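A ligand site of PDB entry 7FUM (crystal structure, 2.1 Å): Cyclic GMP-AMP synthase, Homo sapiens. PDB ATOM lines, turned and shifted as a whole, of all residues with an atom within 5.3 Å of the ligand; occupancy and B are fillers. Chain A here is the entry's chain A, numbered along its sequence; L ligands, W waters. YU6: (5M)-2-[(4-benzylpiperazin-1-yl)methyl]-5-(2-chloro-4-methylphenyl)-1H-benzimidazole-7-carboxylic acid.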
ATOM      1  N   LEU A  49       3.145   6.159  24.347  1.00  0.00           N
ATOM      2  CA  LEU A  49       2.263   6.494  25.466  1.00  0.00           C
ATOM      3  C   LEU A  49       0.837   6.277  24.977  1.00  0.00           C
ATOM      4  O   LEU A  49       0.486   6.799  23.913  1.00  0.00           O
ATOM      5  CB  LEU A  49       2.484   7.909  26.009  1.00  0.00           C
ATOM      6  CG  LEU A  49       1.681   8.226  27.282  1.00  0.00           C
ATOM      7  CD1 LEU A  49       2.025   7.272  28.430  1.00  0.00           C
ATOM      8  CD2 LEU A  49       1.849   9.675  27.701  1.00  0.00           C
ATOM      9  N   ASN A  50       0.048   5.465  25.719  1.00  0.00           N
ATOM     10  CA  ASN A  50      -1.315   4.989  25.420  1.00  0.00           C
ATOM     11  C   ASN A  50      -1.268   4.145  24.126  1.00  0.00           C
ATOM     12  O   ASN A  50      -1.685   4.574  23.039  1.00  0.00           O
ATOM     13  CB  ASN A  50      -2.440   6.073  25.479  1.00  0.00           C
ATOM     14  CG  ASN A  50      -2.519   7.138  24.384  1.00  0.00           C
ATOM     15  OD1 ASN A  50      -3.230   6.985  23.382  1.00  0.00           O
ATOM     16  ND2 ASN A  50      -1.839   8.251  24.587  1.00  0.00           N
ATOM     17  N   TYR A  55      -5.517   6.839  18.681  1.00  0.00           N
ATOM     18  CA  TYR A  55      -4.226   7.534  18.541  1.00  0.00           C
ATOM     19  C   TYR A  55      -4.154   9.010  19.020  1.00  0.00           C
ATOM     20  O   TYR A  55      -3.030   9.484  19.159  1.00  0.00           O
ATOM     21  CB  TYR A  55      -3.646   7.432  17.118  1.00  0.00           C
ATOM     22  CG  TYR A  55      -2.733   6.231  16.981  1.00  0.00           C
ATOM     23  CD1 TYR A  55      -1.529   6.159  17.683  1.00  0.00           C
ATOM     24  CD2 TYR A  55      -3.100   5.137  16.213  1.00  0.00           C
ATOM     25  CE1 TYR A  55      -0.708   5.044  17.605  1.00  0.00           C
ATOM     26  CE2 TYR A  55      -2.290   4.008  16.124  1.00  0.00           C
ATOM     27  CZ  TYR A  55      -1.087   3.971  16.821  1.00  0.00           C
ATOM     28  OH  TYR A  55      -0.267   2.872  16.741  1.00  0.00           O
ATOM     29  N   GLU A  56      -5.282   9.673  19.337  1.00  0.00           N
ATOM     30  CA  GLU A  56      -5.364  11.091  19.776  1.00  0.00           C
ATOM     31  C   GLU A  56      -5.209  12.067  18.600  1.00  0.00           C
ATOM     32  O   GLU A  56      -4.313  11.898  17.768  1.00  0.00           O
ATOM     33  CB  GLU A  56      -4.403  11.473  20.941  1.00  0.00           C
ATOM     34  CG  GLU A  56      -4.399  10.531  22.144  1.00  0.00           C
ATOM     35  CD  GLU A  56      -5.119  11.007  23.399  1.00  0.00           C
ATOM     36  OE1 GLU A  56      -6.352  11.209  23.343  1.00  0.00           O
ATOM     37  OE2 GLU A  56      -4.444  11.152  24.446  1.00  0.00           O
ATOM     38  N   VAL A  58      -5.143  16.342  17.368  1.00  0.00           N
ATOM     39  CA  VAL A  58      -4.908  17.725  17.803  1.00  0.00           C
ATOM     40  C   VAL A  58      -6.117  18.620  17.425  1.00  0.00           C
ATOM     41  O   VAL A  58      -6.361  19.621  18.104  1.00  0.00           O
ATOM     42  CB  VAL A  58      -3.561  18.348  17.319  1.00  0.00           C
ATOM     43  CG1 VAL A  58      -2.894  19.144  18.437  1.00  0.00           C
ATOM     44  CG2 VAL A  58      -2.607  17.299  16.736  1.00  0.00           C
ATOM     45  N   ASP A  67      -1.884  12.908  16.640  1.00  0.00           N
ATOM     46  CA  ASP A  67      -0.968  13.350  17.696  1.00  0.00           C
ATOM     47  C   ASP A  67      -0.403  12.130  18.447  1.00  0.00           C
ATOM     48  O   ASP A  67      -1.179  11.412  19.056  1.00  0.00           O
ATOM     49  CB  ASP A  67      -1.745  14.256  18.648  1.00  0.00           C
ATOM     50  CG  ASP A  67      -0.903  15.011  19.625  1.00  0.00           C
ATOM     51  OD1 ASP A  67       0.278  15.276  19.306  1.00  0.00           O
ATOM     52  OD2 ASP A  67      -1.408  15.315  20.712  1.00  0.00           O
ATOM     53  N   VAL A  68       0.910  11.854  18.365  1.00  0.00           N
ATOM     54  CA  VAL A  68       1.433  10.671  19.054  1.00  0.00           C
ATOM     55  C   VAL A  68       2.647  11.029  19.919  1.00  0.00           C
ATOM     56  O   VAL A  68       3.397  11.957  19.622  1.00  0.00           O
ATOM     57  CB  VAL A  68       1.663   9.385  18.162  1.00  0.00           C
ATOM     58  CG1 VAL A  68       0.684   9.281  16.985  1.00  0.00           C
ATOM     59  CG2 VAL A  68       3.096   9.188  17.709  1.00  0.00           C
ATOM     60  N   MET A  69       2.801  10.269  21.007  1.00  0.00           N
ATOM     61  CA  MET A  69       3.914  10.419  21.916  1.00  0.00           C
ATOM     62  C   MET A  69       4.702   9.148  22.166  1.00  0.00           C
ATOM     63  O   MET A  69       4.149   8.110  22.502  1.00  0.00           O
ATOM     64  CB  MET A  69       3.517  11.031  23.265  1.00  0.00           C
ATOM     65  CG  MET A  69       4.750  11.267  24.173  1.00  0.00           C
ATOM     66  SD  MET A  69       4.422  11.428  25.935  1.00  0.00           S
ATOM     67  CE  MET A  69       3.985  13.177  25.981  1.00  0.00           C
ATOM     68  N   THR A 161       5.912  13.460  19.341  1.00  0.00           N
ATOM     69  CA  THR A 161       6.637  14.115  20.430  1.00  0.00           C
ATOM     70  C   THR A 161       7.403  13.043  21.190  1.00  0.00           C
ATOM     71  O   THR A 161       6.856  11.984  21.491  1.00  0.00           O
ATOM     72  CB  THR A 161       5.674  14.850  21.424  1.00  0.00           C
ATOM     73  OG1 THR A 161       4.753  15.721  20.733  1.00  0.00           O
ATOM     74  CG2 THR A 161       6.430  15.663  22.470  1.00  0.00           C
ATOM     75  N   LEU A 178      -3.912  22.040  39.713  1.00  0.00           N
ATOM     76  CA  LEU A 178      -4.969  21.023  39.687  1.00  0.00           C
ATOM     77  C   LEU A 178      -6.017  21.252  40.842  1.00  0.00           C
ATOM     78  O   LEU A 178      -6.286  20.370  41.651  1.00  0.00           O
ATOM     79  CB  LEU A 178      -4.345  19.611  39.671  1.00  0.00           C
ATOM     80  CG  LEU A 178      -5.283  18.428  39.453  1.00  0.00           C
ATOM     81  CD1 LEU A 178      -5.859  18.404  38.017  1.00  0.00           C
ATOM     82  CD2 LEU A 178      -4.571  17.147  39.830  1.00  0.00           C
ATOM     83  N   ARG A 216      10.105  21.081  29.371  1.00  0.00           N
ATOM     84  CA  ARG A 216       8.852  21.599  29.902  1.00  0.00           C
ATOM     85  C   ARG A 216       8.046  20.488  30.587  1.00  0.00           C
ATOM     86  O   ARG A 216       7.883  19.409  30.014  1.00  0.00           O
ATOM     87  CB  ARG A 216       8.037  22.275  28.763  1.00  0.00           C
ATOM     88  CG  ARG A 216       6.770  22.973  29.250  1.00  0.00           C
ATOM     89  CD  ARG A 216       5.801  23.417  28.162  1.00  0.00           C
ATOM     90  NE  ARG A 216       5.351  22.350  27.268  1.00  0.00           N
ATOM     91  CZ  ARG A 216       4.301  21.536  27.453  1.00  0.00           C
ATOM     92  NH1 ARG A 216       3.586  21.616  28.580  1.00  0.00           N
ATOM     93  NH2 ARG A 216       3.968  20.640  26.548  1.00  0.00           N
ATOM     94  N   LEU A 217       7.480  20.774  31.777  1.00  0.00           N
ATOM     95  CA  LEU A 217       6.599  19.847  32.511  1.00  0.00           C
ATOM     96  C   LEU A 217       5.294  19.727  31.756  1.00  0.00           C
ATOM     97  O   LEU A 217       4.636  20.736  31.464  1.00  0.00           O
ATOM     98  CB  LEU A 217       6.253  20.362  33.914  1.00  0.00           C
ATOM     99  CG  LEU A 217       7.342  20.507  34.967  1.00  0.00           C
ATOM    100  CD1 LEU A 217       6.706  20.989  36.284  1.00  0.00           C
ATOM    101  CD2 LEU A 217       8.095  19.171  35.183  1.00  0.00           C
ATOM    102  N   SER A 218       4.895  18.483  31.497  1.00  0.00           N
ATOM    103  CA  SER A 218       3.667  18.168  30.782  1.00  0.00           C
ATOM    104  C   SER A 218       2.755  17.220  31.591  1.00  0.00           C
ATOM    105  O   SER A 218       3.207  16.221  32.152  1.00  0.00           O
ATOM    106  CB  SER A 218       4.013  17.537  29.431  1.00  0.00           C
ATOM    107  OG  SER A 218       2.845  17.373  28.653  1.00  0.00           O
ATOM    108  N   PHE A 219       1.474  17.564  31.649  1.00  0.00           N
ATOM    109  CA  PHE A 219       0.484  16.735  32.326  1.00  0.00           C
ATOM    110  C   PHE A 219      -0.671  16.447  31.351  1.00  0.00           C
ATOM    111  O   PHE A 219      -1.775  16.272  31.801  1.00  0.00           O
ATOM    112  CB  PHE A 219      -0.048  17.469  33.578  1.00  0.00           C
ATOM    113  CG  PHE A 219       1.034  17.805  34.584  1.00  0.00           C
ATOM    114  CD1 PHE A 219       1.476  16.857  35.491  1.00  0.00           C
ATOM    115  CD2 PHE A 219       1.659  19.052  34.576  1.00  0.00           C
ATOM    116  CE1 PHE A 219       2.511  17.147  36.375  1.00  0.00           C
ATOM    117  CE2 PHE A 219       2.689  19.349  35.474  1.00  0.00           C
ATOM    118  CZ  PHE A 219       3.110  18.391  36.358  1.00  0.00           C
ATOM    119  N   SER A 220      -0.415  16.409  30.017  1.00  0.00           N
ATOM    120  CA  SER A 220      -1.473  16.202  28.973  1.00  0.00           C
ATOM    121  C   SER A 220      -2.297  14.896  29.200  1.00  0.00           C
ATOM    122  O   SER A 220      -3.496  14.870  28.905  1.00  0.00           O
ATOM    123  CB  SER A 220      -0.872  16.216  27.573  1.00  0.00           C
ATOM    124  OG  SER A 220       0.036  15.137  27.398  1.00  0.00           O
ATOM    125  N   ILE A 222      -3.386  13.709  31.964  1.00  0.00           N
ATOM    126  CA  ILE A 222      -4.369  13.850  33.051  1.00  0.00           C
ATOM    127  C   ILE A 222      -5.746  14.216  32.470  1.00  0.00           C
ATOM    128  O   ILE A 222      -6.768  13.952  33.105  1.00  0.00           O
ATOM    129  CB  ILE A 222      -3.868  14.827  34.180  1.00  0.00           C
ATOM    130  CG1 ILE A 222      -2.547  14.333  34.828  1.00  0.00           C
ATOM    131  CG2 ILE A 222      -4.938  15.106  35.275  1.00  0.00           C
ATOM    132  CD1 ILE A 222      -2.618  12.997  35.716  1.00  0.00           C
ATOM    133  N   GLU A 223      -5.771  14.827  31.273  1.00  0.00           N
ATOM    134  CA  GLU A 223      -7.025  15.239  30.645  1.00  0.00           C
ATOM    135  C   GLU A 223      -8.064  14.104  30.427  1.00  0.00           C
ATOM    136  O   GLU A 223      -9.234  14.296  30.760  1.00  0.00           O
ATOM    137  CB  GLU A 223      -6.736  15.939  29.325  1.00  0.00           C
ATOM    138  CG  GLU A 223      -7.921  16.723  28.855  1.00  0.00           C
ATOM    139  CD  GLU A 223      -7.876  17.142  27.415  1.00  0.00           C
ATOM    140  OE1 GLU A 223      -6.880  16.866  26.715  1.00  0.00           O
ATOM    141  OE2 GLU A 223      -8.861  17.787  26.981  1.00  0.00           O
ATOM    142  N   ILE A 226      -9.764  12.955  33.695  1.00  0.00           N
ATOM    143  CA  ILE A 226     -10.788  13.869  34.158  1.00  0.00           C
ATOM    144  C   ILE A 226     -11.986  13.864  33.225  1.00  0.00           C
ATOM    145  O   ILE A 226     -13.101  13.792  33.707  1.00  0.00           O
ATOM    146  CB  ILE A 226     -10.207  15.271  34.415  1.00  0.00           C
ATOM    147  CG1 ILE A 226      -9.273  15.174  35.666  1.00  0.00           C
ATOM    148  CG2 ILE A 226     -11.354  16.329  34.548  1.00  0.00           C
ATOM    149  CD1 ILE A 226      -8.812  16.379  36.370  1.00  0.00           C
ATOM    150  N   TYR A 276      -4.792  23.832  23.391  1.00  0.00           N
ATOM    151  CA  TYR A 276      -4.263  23.821  24.746  1.00  0.00           C
ATOM    152  C   TYR A 276      -4.738  25.044  25.582  1.00  0.00           C
ATOM    153  O   TYR A 276      -5.160  24.871  26.740  1.00  0.00           O
ATOM    154  CB  TYR A 276      -2.737  23.761  24.691  1.00  0.00           C
ATOM    155  CG  TYR A 276      -2.084  23.877  26.046  1.00  0.00           C
ATOM    156  CD1 TYR A 276      -2.422  23.011  27.093  1.00  0.00           C
ATOM    157  CD2 TYR A 276      -1.100  24.838  26.293  1.00  0.00           C
ATOM    158  CE1 TYR A 276      -1.770  23.075  28.324  1.00  0.00           C
ATOM    159  CE2 TYR A 276      -0.467  24.926  27.532  1.00  0.00           C
ATOM    160  CZ  TYR A 276      -0.800  24.038  28.544  1.00  0.00           C
ATOM    161  OH  TYR A 276      -0.194  24.124  29.775  1.00  0.00           O
ATOM    162  N   LYS A 279      -8.516  24.396  26.180  1.00  0.00           N
ATOM    163  CA  LYS A 279      -8.633  23.361  27.204  1.00  0.00           C
ATOM    164  C   LYS A 279      -8.416  23.932  28.603  1.00  0.00           C
ATOM    165  O   LYS A 279      -9.235  23.691  29.483  1.00  0.00           O
ATOM    166  CB  LYS A 279      -7.596  22.264  26.982  1.00  0.00           C
ATOM    167  CG  LYS A 279      -7.895  21.358  25.808  1.00  0.00           C
ATOM    168  CD  LYS A 279      -6.836  20.306  25.831  1.00  0.00           C
ATOM    169  CE  LYS A 279      -6.509  19.716  24.486  1.00  0.00           C
ATOM    170  NZ  LYS A 279      -5.676  18.485  24.677  1.00  0.00           N
ATOM    171  N   THR A 280      -7.304  24.682  28.801  1.00  0.00           N
ATOM    172  CA  THR A 280      -6.908  25.307  30.066  1.00  0.00           C
ATOM    173  C   THR A 280      -8.028  26.192  30.605  1.00  0.00           C
ATOM    174  O   THR A 280      -8.452  25.969  31.734  1.00  0.00           O
ATOM    175  CB  THR A 280      -5.585  26.084  29.923  1.00  0.00           C
ATOM    176  OG1 THR A 280      -4.576  25.206  29.429  1.00  0.00           O
ATOM    177  CG2 THR A 280      -5.111  26.710  31.223  1.00  0.00           C
ATOM    178  N   PHE A 283     -11.142  24.142  31.689  1.00  0.00           N
ATOM    179  CA  PHE A 283     -10.975  23.470  32.995  1.00  0.00           C
ATOM    180  C   PHE A 283     -10.993  24.467  34.159  1.00  0.00           C
ATOM    181  O   PHE A 283     -11.431  24.088  35.254  1.00  0.00           O
ATOM    182  CB  PHE A 283      -9.772  22.518  33.032  1.00  0.00           C
ATOM    183  CG  PHE A 283     -10.041  21.251  32.252  1.00  0.00           C
ATOM    184  CD1 PHE A 283     -10.983  20.323  32.685  1.00  0.00           C
ATOM    185  CD2 PHE A 283      -9.365  21.002  31.054  1.00  0.00           C
ATOM    186  CE1 PHE A 283     -11.245  19.162  31.954  1.00  0.00           C
ATOM    187  CE2 PHE A 283      -9.619  19.819  30.325  1.00  0.00           C
ATOM    188  CZ  PHE A 283     -10.555  18.911  30.784  1.00  0.00           C
ATOM    189  N   ASN A 322      -1.424  28.204  33.810  1.00  0.00           N
ATOM    190  CA  ASN A 322      -1.275  26.789  33.509  1.00  0.00           C
ATOM    191  C   ASN A 322      -2.124  26.111  34.617  1.00  0.00           C
ATOM    192  O   ASN A 322      -2.022  26.502  35.788  1.00  0.00           O
ATOM    193  CB  ASN A 322       0.181  26.398  33.661  1.00  0.00           C
ATOM    194  CG  ASN A 322       0.476  24.962  33.375  1.00  0.00           C
ATOM    195  OD1 ASN A 322      -0.135  24.050  33.932  1.00  0.00           O
ATOM    196  ND2 ASN A 322       1.473  24.727  32.545  1.00  0.00           N
ATOM    197  N   TYR A 323      -3.007  25.162  34.216  1.00  0.00           N
ATOM    198  CA  TYR A 323      -3.923  24.476  35.113  1.00  0.00           C
ATOM    199  C   TYR A 323      -3.188  23.720  36.244  1.00  0.00           C
ATOM    200  O   TYR A 323      -3.728  23.543  37.355  1.00  0.00           O
ATOM    201  CB  TYR A 323      -4.830  23.547  34.291  1.00  0.00           C
ATOM    202  CG  TYR A 323      -6.095  23.195  35.034  1.00  0.00           C
ATOM    203  CD1 TYR A 323      -7.086  24.160  35.264  1.00  0.00           C
ATOM    204  CD2 TYR A 323      -6.265  21.943  35.624  1.00  0.00           C
ATOM    205  CE1 TYR A 323      -8.195  23.885  36.058  1.00  0.00           C
ATOM    206  CE2 TYR A 323      -7.395  21.644  36.375  1.00  0.00           C
ATOM    207  CZ  TYR A 323      -8.368  22.606  36.573  1.00  0.00           C
ATOM    208  OH  TYR A 323      -9.495  22.333  37.304  1.00  0.00           O
ATOM    209  N   PHE A 324      -1.937  23.332  35.987  1.00  0.00           N
ATOM    210  CA  PHE A 324      -1.074  22.601  36.919  1.00  0.00           C
ATOM    211  C   PHE A 324       0.011  23.463  37.574  1.00  0.00           C
ATOM    212  O   PHE A 324       0.573  23.063  38.575  1.00  0.00           O
ATOM    213  CB  PHE A 324      -0.387  21.440  36.175  1.00  0.00           C
ATOM    214  CG  PHE A 324      -1.377  20.378  35.740  1.00  0.00           C
ATOM    215  CD1 PHE A 324      -2.159  20.553  34.598  1.00  0.00           C
ATOM    216  CD2 PHE A 324      -1.549  19.218  36.501  1.00  0.00           C
ATOM    217  CE1 PHE A 324      -3.108  19.608  34.240  1.00  0.00           C
ATOM    218  CE2 PHE A 324      -2.493  18.265  36.128  1.00  0.00           C
ATOM    219  CZ  PHE A 324      -3.286  18.473  35.013  1.00  0.00           C
HETATM  220  C10 YU6 L   1       0.204  12.803  22.054  1.00  0.00           C
HETATM  221  C11 YU6 L   1      -0.370  11.566  22.342  1.00  0.00           C
HETATM  222  C13 YU6 L   1       0.264  11.811  24.640  1.00  0.00           C
HETATM  223  C15 YU6 L   1      -1.793  19.738  25.467  1.00  0.00           C
HETATM  224  C17 YU6 L   1      -1.517  19.676  27.658  1.00  0.00           C
HETATM  225  C18 YU6 L   1      -2.861  19.481  27.323  1.00  0.00           C
HETATM  226  C20 YU6 L   1      -3.828  19.342  28.315  1.00  0.00           C
HETATM  227  C21 YU6 L   1      -3.451  19.394  29.665  1.00  0.00           C
HETATM  228  C22 YU6 L   1      -4.484  19.304  30.738  1.00  0.00           C
HETATM  229  C23 YU6 L   1      -5.287  20.396  31.114  1.00  0.00           C
HETATM  230  C25 YU6 L   1      -6.223  20.300  32.116  1.00  0.00           C
HETATM  231  C26 YU6 L   1      -6.436  19.083  32.762  1.00  0.00           C
HETATM  232  C27 YU6 L   1      -7.459  18.950  33.860  1.00  0.00           C
HETATM  233  C28 YU6 L   1      -5.649  17.986  32.390  1.00  0.00           C
HETATM  234  C1  YU6 L   1      -1.417  19.662  24.026  1.00  0.00           C
HETATM  235  C12 YU6 L   1      -0.338  11.072  23.631  1.00  0.00           C
HETATM  236  C14 YU6 L   1       0.829  13.053  24.352  1.00  0.00           C
HETATM  237  C29 YU6 L   1      -4.694  18.089  31.397  1.00  0.00           C
HETATM  238  C3  YU6 L   1      -0.016  18.461  22.427  1.00  0.00           C
HETATM  239  C30 YU6 L   1      -2.131  19.732  29.992  1.00  0.00           C
HETATM  240  C31 YU6 L   1      -1.132  19.739  29.004  1.00  0.00           C
HETATM  241  C32 YU6 L   1       0.294  19.945  29.452  1.00  0.00           C
HETATM  242  C4  YU6 L   1       0.982  17.290  22.319  1.00  0.00           C
HETATM  243  C6  YU6 L   1      -0.422  16.056  23.930  1.00  0.00           C
HETATM  244  C7  YU6 L   1      -1.383  17.231  23.920  1.00  0.00           C
HETATM  245  C8  YU6 L   1       1.390  14.921  22.753  1.00  0.00           C
HETATM  246  C9  YU6 L   1       0.830  13.541  23.058  1.00  0.00           C
HETATM  247  N16 YU6 L   1      -0.851  19.786  26.449  1.00  0.00           N
HETATM  248  N19 YU6 L   1      -3.005  19.527  25.938  1.00  0.00           N
HETATM  249  N2  YU6 L   1      -0.620  18.474  23.759  1.00  0.00           N
HETATM  250  N5  YU6 L   1       0.365  15.979  22.671  1.00  0.00           N
HETATM  251  O33 YU6 L   1       1.154  20.071  28.564  1.00  0.00           O
HETATM  252  O34 YU6 L   1       0.539  20.036  30.693  1.00  0.00           O
HETATM  253 CL24 YU6 L   1      -5.110  21.926  30.293  1.00  0.00          CL
HETATM  254  O   HOH W   1      -0.784  22.403  31.827  1.00  0.00           O
HETATM  255  O   HOH W   2      -1.846  12.906  26.528  1.00  0.00           O
HETATM  256  O   HOH W   3       2.290  21.965  32.005  1.00  0.00           O
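A nitrogen (N5) of the ligand lies within salt-bridge range of the side-chain carboxylate (OD2) of Asp 67 (2.7 Å). O34 of the ligand sits at hydrogen-bond distance from N of Phe 219 (2.8 Å). An oxygen (O33) of the ligand lies within salt-bridge range of the guanidinium group of Arg 216. The side-chain amino group (NZ) of Lys 279 lies within hydrogen-bond range of a nitrogen (N19) of the ligand. OG of Ser 218 is in hydrogen-bond range of O33 of the ligand (3.2 Å).
The backbone carbonyl oxygen of Glu 56 sits at hydrogen-bond distance from the backbone NH of Asp 67 (2.9 Å). O of Asp 67 sits close to O of Tyr 55 (2.7 Å). The side-chain hydroxyl (OH) of Tyr 323 sits at hydrogen-bond distance from the backbone carbonyl oxygen (O) of Phe 283 (3.3 Å). O of Tyr 276 sits at hydrogen-bond distance from OG1 of Thr 280. The side-chain hydroxyl (OH) of Tyr 276 is in hydrogen-bond range of the side-chain amide nitrogen (ND2) of Asn 322 (3.3 Å). The backbone NH (N) of Leu 49 lies within hydrogen-bond range of the backbone carbonyl oxygen (O) of Met 69, 2.9 Å away. O of Tyr 323 sits at hydrogen-bond distance from N of Leu 178, at 2.8 Å. The backbone NH (N) of Thr 161 lies within hydrogen-bond range of the backbone carbonyl oxygen (O) of Val 68 (2.9 Å).
Merely in contact with the ligand: Asn 50 (3.3 Å), Glu 223 (3.4 Å), Phe 283 (3.4 Å), Thr 280 (3.4 Å), Tyr 276 (3.5 Å), Ser 220 (3.5 Å), Met 69 (3.5 Å), Phe 324 (3.5 Å), Tyr 323 (3.7 Å), Val 68 (3.7 Å), Ile 222 (3.8 Å) and Ile 226 (3.8 Å). Hydrophobic or aromatic side chains within 4 Å of the ligand: Met 69, Phe 219, Ile 226, Tyr 276, Phe 283, Tyr 323 and Phe 324. Of the 25 residues printed, 17 come within 4 Å of the ligand.
Water W3 lies within hydrogen-bond range of O of Leu 217, O34 of the ligand and ND2 of Asn 322. Water W1 lies within hydrogen-bond range of the side-chain hydroxyl of Tyr 276 (2.7 Å), the side-chain amide oxygen of Asn 322 (2.8 Å) and an oxygen (O34) of the ligand (2.9 Å).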
